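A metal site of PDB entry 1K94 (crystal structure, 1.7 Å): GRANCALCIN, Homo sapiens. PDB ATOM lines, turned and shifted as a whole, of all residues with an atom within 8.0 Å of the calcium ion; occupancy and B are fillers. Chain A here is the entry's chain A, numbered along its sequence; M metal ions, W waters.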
ATOM      1  N   PHE A   6      28.368  31.430  -0.417  1.00  0.00           N
ATOM      2  CA  PHE A   6      28.241  31.525  -1.873  1.00  0.00           C
ATOM      3  C   PHE A   6      29.638  31.604  -2.468  1.00  0.00           C
ATOM      4  O   PHE A   6      29.979  30.883  -3.405  1.00  0.00           O
ATOM      5  CB  PHE A   6      27.460  32.788  -2.253  1.00  0.00           C
ATOM      6  CG  PHE A   6      27.226  32.940  -3.732  1.00  0.00           C
ATOM      7  CD1 PHE A   6      26.050  32.465  -4.320  1.00  0.00           C
ATOM      8  CD2 PHE A   6      28.195  33.523  -4.547  1.00  0.00           C
ATOM      9  CE1 PHE A   6      25.843  32.593  -5.700  1.00  0.00           C
ATOM     10  CE2 PHE A   6      27.988  33.650  -5.927  1.00  0.00           C
ATOM     11  CZ  PHE A   6      26.809  33.175  -6.505  1.00  0.00           C
ATOM     12  N   VAL A   9      31.590  28.265  -2.337  1.00  0.00           N
ATOM     13  CA  VAL A   9      31.169  27.203  -3.238  1.00  0.00           C
ATOM     14  C   VAL A   9      31.154  27.610  -4.704  1.00  0.00           C
ATOM     15  O   VAL A   9      31.039  26.751  -5.583  1.00  0.00           O
ATOM     16  CB  VAL A   9      29.751  26.689  -2.897  1.00  0.00           C
ATOM     17  CG1 VAL A   9      29.711  26.153  -1.476  1.00  0.00           C
ATOM     18  CG2 VAL A   9      28.740  27.820  -3.078  1.00  0.00           C
ATOM     19  N   ALA A  10      31.282  28.903  -4.960  1.00  0.00           N
ATOM     20  CA  ALA A  10      31.240  29.437  -6.320  1.00  0.00           C
ATOM     21  C   ALA A  10      32.237  28.824  -7.297  1.00  0.00           C
ATOM     22  O   ALA A  10      31.933  28.651  -8.476  1.00  0.00           O
ATOM     23  CB  ALA A  10      31.421  30.951  -6.288  1.00  0.00           C
ATOM     24  N   GLY A  11      33.437  28.526  -6.821  1.00  0.00           N
ATOM     25  CA  GLY A  11      34.432  27.944  -7.713  1.00  0.00           C
ATOM     26  C   GLY A  11      35.118  28.986  -8.568  1.00  0.00           C
ATOM     27  O   GLY A  11      34.908  30.183  -8.381  1.00  0.00           O
ATOM     28  N   GLN A  12      35.906  28.508  -9.527  1.00  0.00           N
ATOM     29  CA  GLN A  12      36.675  29.380 -10.414  1.00  0.00           C
ATOM     30  C   GLN A  12      35.898  30.366 -11.290  1.00  0.00           C
ATOM     31  O   GLN A  12      36.455  31.375 -11.704  1.00  0.00           O
ATOM     32  CB  GLN A  12      37.581  28.522 -11.308  1.00  0.00           C
ATOM     33  CG  GLN A  12      38.364  27.444 -10.551  1.00  0.00           C
ATOM     34  CD  GLN A  12      39.390  28.002  -9.571  1.00  0.00           C
ATOM     35  OE1 GLN A  12      39.935  27.259  -8.748  1.00  0.00           O
ATOM     36  NE2 GLN A  12      39.666  29.295  -9.665  1.00  0.00           N
ATOM     37  N   ASP A  13      34.635  30.082 -11.586  1.00  0.00           N
ATOM     38  CA  ASP A  13      33.875  31.003 -12.431  1.00  0.00           C
ATOM     39  C   ASP A  13      33.018  32.020 -11.669  1.00  0.00           C
ATOM     40  O   ASP A  13      32.281  32.794 -12.270  1.00  0.00           O
ATOM     41  CB  ASP A  13      33.005  30.222 -13.428  1.00  0.00           C
ATOM     42  CG  ASP A  13      31.873  29.475 -12.771  1.00  0.00           C
ATOM     43  OD1 ASP A  13      31.905  29.260 -11.546  1.00  0.00           O
ATOM     44  OD2 ASP A  13      30.935  29.080 -13.498  1.00  0.00           O
ATOM     45  N   GLY A  14      33.115  32.016 -10.339  1.00  0.00           N
ATOM     46  CA  GLY A  14      32.379  32.967  -9.529  1.00  0.00           C
ATOM     47  C   GLY A  14      30.862  32.917  -9.595  1.00  0.00           C
ATOM     48  O   GLY A  14      30.186  33.851  -9.174  1.00  0.00           O
ATOM     49  N   GLU A  15      30.329  31.826 -10.122  1.00  0.00           N
ATOM     50  CA  GLU A  15      28.881  31.648 -10.231  1.00  0.00           C
ATOM     51  C   GLU A  15      28.536  30.238  -9.770  1.00  0.00           C
ATOM     52  O   GLU A  15      29.402  29.362  -9.754  1.00  0.00           O
ATOM     53  CB  GLU A  15      28.432  31.856 -11.679  1.00  0.00           C
ATOM     54  CG  GLU A  15      28.884  33.189 -12.284  1.00  0.00           C
ATOM     55  CD  GLU A  15      28.216  33.497 -13.615  1.00  0.00           C
ATOM     56  OE1 GLU A  15      28.020  32.550 -14.418  1.00  0.00           O
ATOM     57  OE2 GLU A  15      27.896  34.676 -13.872  1.00  0.00           O
ATOM     58  N   VAL A  16      27.278  30.009  -9.398  1.00  0.00           N
ATOM     59  CA  VAL A  16      26.912  28.682  -8.926  1.00  0.00           C
ATOM     60  C   VAL A  16      25.996  27.896  -9.863  1.00  0.00           C
ATOM     61  O   VAL A  16      25.120  28.464 -10.505  1.00  0.00           O
ATOM     62  CB  VAL A  16      26.192  28.743  -7.535  1.00  0.00           C
ATOM     63  CG1 VAL A  16      27.140  29.335  -6.490  1.00  0.00           C
ATOM     64  CG2 VAL A  16      24.919  29.576  -7.639  1.00  0.00           C
ATOM     65  N   ASP A  17      26.245  26.597  -9.954  1.00  0.00           N
ATOM     66  CA  ASP A  17      25.376  25.741 -10.749  1.00  0.00           C
ATOM     67  C   ASP A  17      24.470  25.093  -9.715  1.00  0.00           C
ATOM     68  O   ASP A  17      24.538  25.429  -8.534  1.00  0.00           O
ATOM     69  CB  ASP A  17      26.188  24.709 -11.555  1.00  0.00           C
ATOM     70  CG  ASP A  17      27.083  23.832 -10.703  1.00  0.00           C
ATOM     71  OD1 ASP A  17      27.931  23.124 -11.290  1.00  0.00           O
ATOM     72  OD2 ASP A  17      26.952  23.832  -9.453  1.00  0.00           O
ATOM     73  N   ALA A  18      23.607  24.175 -10.130  1.00  0.00           N
ATOM     74  CA  ALA A  18      22.672  23.551  -9.185  1.00  0.00           C
ATOM     75  C   ALA A  18      23.349  22.916  -7.968  1.00  0.00           C
ATOM     76  O   ALA A  18      22.914  23.116  -6.824  1.00  0.00           O
ATOM     77  CB  ALA A  18      21.819  22.508  -9.896  1.00  0.00           C
ATOM     78  N   GLU A  19      24.405  22.161  -8.225  1.00  0.00           N
ATOM     79  CA  GLU A  19      25.137  21.460  -7.174  1.00  0.00           C
ATOM     80  C   GLU A  19      25.817  22.421  -6.183  1.00  0.00           C
ATOM     81  O   GLU A  19      25.795  22.203  -4.972  1.00  0.00           O
ATOM     82  CB  GLU A  19      26.154  20.533  -7.837  1.00  0.00           C
ATOM     83  CG  GLU A  19      26.969  19.660  -6.902  1.00  0.00           C
ATOM     84  CD  GLU A  19      28.115  20.399  -6.251  1.00  0.00           C
ATOM     85  OE1 GLU A  19      28.806  21.164  -6.959  1.00  0.00           O
ATOM     86  OE2 GLU A  19      28.319  20.217  -5.041  1.00  0.00           O
ATOM     87  N   GLU A  20      26.408  23.488  -6.709  1.00  0.00           N
ATOM     88  CA  GLU A  20      27.082  24.470  -5.862  1.00  0.00           C
ATOM     89  C   GLU A  20      26.039  25.224  -5.043  1.00  0.00           C
ATOM     90  O   GLU A  20      26.240  25.483  -3.853  1.00  0.00           O
ATOM     91  CB  GLU A  20      27.871  25.442  -6.737  1.00  0.00           C
ATOM     92  CG  GLU A  20      29.111  24.810  -7.352  1.00  0.00           C
ATOM     93  CD  GLU A  20      29.728  25.655  -8.436  1.00  0.00           C
ATOM     94  OE1 GLU A  20      30.927  25.464  -8.729  1.00  0.00           O
ATOM     95  OE2 GLU A  20      29.025  26.501  -9.012  1.00  0.00           O
ATOM     96  N   LEU A  21      24.928  25.557  -5.669  1.00  0.00           N
ATOM     97  CA  LEU A  21      23.851  26.259  -4.987  1.00  0.00           C
ATOM     98  C   LEU A  21      23.319  25.417  -3.839  1.00  0.00           C
ATOM     99  O   LEU A  21      23.052  25.935  -2.752  1.00  0.00           O
ATOM    100  CB  LEU A  21      22.709  26.575  -5.964  1.00  0.00           C
ATOM    101  CG  LEU A  21      21.486  27.280  -5.371  1.00  0.00           C
ATOM    102  CD1 LEU A  21      21.896  28.581  -4.694  1.00  0.00           C
ATOM    103  CD2 LEU A  21      20.475  27.547  -6.473  1.00  0.00           C
ATOM    104  N   ARG A  23      24.905  23.270  -2.092  1.00  0.00           N
ATOM    105  CA  ARG A  23      25.884  23.307  -1.006  1.00  0.00           C
ATOM    106  C   ARG A  23      25.784  24.628  -0.233  1.00  0.00           C
ATOM    107  O   ARG A  23      25.812  24.632   0.997  1.00  0.00           O
ATOM    108  CB  ARG A  23      27.297  23.145  -1.563  1.00  0.00           C
ATOM    109  CG  ARG A  23      27.695  21.702  -1.833  1.00  0.00           C
ATOM    110  CD  ARG A  23      29.166  21.602  -2.174  1.00  0.00           C
ATOM    111  NE  ARG A  23      29.451  22.058  -3.537  1.00  0.00           N
ATOM    112  CZ  ARG A  23      30.524  22.763  -3.881  1.00  0.00           C
ATOM    113  NH1 ARG A  23      31.417  23.116  -2.972  1.00  0.00           N
ATOM    114  NH2 ARG A  23      30.711  23.101  -5.155  1.00  0.00           N
ATOM    115  N   LYS A  56      23.655  28.729 -14.894  1.00  0.00           N
ATOM    116  CA  LYS A  56      24.332  29.166 -13.682  1.00  0.00           C
ATOM    117  C   LYS A  56      23.701  30.421 -13.103  1.00  0.00           C
ATOM    118  O   LYS A  56      22.938  31.105 -13.779  1.00  0.00           O
ATOM    119  CB  LYS A  56      25.819  29.419 -13.982  1.00  0.00           C
ATOM    120  CG  LYS A  56      26.583  28.161 -14.341  1.00  0.00           C
ATOM    121  CD  LYS A  56      28.072  28.431 -14.433  1.00  0.00           C
ATOM    122  CE  LYS A  56      28.408  29.258 -15.642  1.00  0.00           C
ATOM    123  NZ  LYS A  56      28.196  28.484 -16.892  1.00  0.00           N
ATOM    124  N   MET A  57      24.016  30.726 -11.850  1.00  0.00           N
ATOM    125  CA  MET A  57      23.443  31.895 -11.199  1.00  0.00           C
ATOM    126  C   MET A  57      24.509  32.826 -10.638  1.00  0.00           C
ATOM    127  O   MET A  57      25.373  32.405  -9.864  1.00  0.00           O
ATOM    128  CB  MET A  57      22.503  31.467 -10.076  1.00  0.00           C
ATOM    129  CG  MET A  57      21.799  32.625  -9.367  1.00  0.00           C
ATOM    130  SD  MET A  57      20.794  32.050  -7.971  1.00  0.00           S
ATOM    131  CE  MET A  57      19.393  31.263  -8.816  1.00  0.00           C
HETATM  132 CA    CA M   1      30.828  27.560 -10.166  1.00  0.00          CA
HETATM  133  O   HOH W   1      29.838  27.003 -12.255  1.00  0.00           O
HETATM  134  O   HOH W   2      32.839  26.526 -11.077  1.00  0.00           O
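The calcium ion is bound by O of Ala 10 (2.3 Å), O of Glu 15 (2.3 Å), water W1 (2.4 Å), OE2 of Glu 20 (2.4 Å), water W2 (2.4 Å), OD1 of Asp 13 (2.4 Å) and OE1 of Glu 20 (2.5 Å).
OD2 of Asp 17 is in hydrogen-bond range of N of Glu 20, 2.8 Å away.
Within 4 Å of the calcium ion: Ala 10, Asp 13, Glu 15 and Glu 20. The nearest printed residue that does not touch the calcium ion is Val 16 (4.3 Å).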
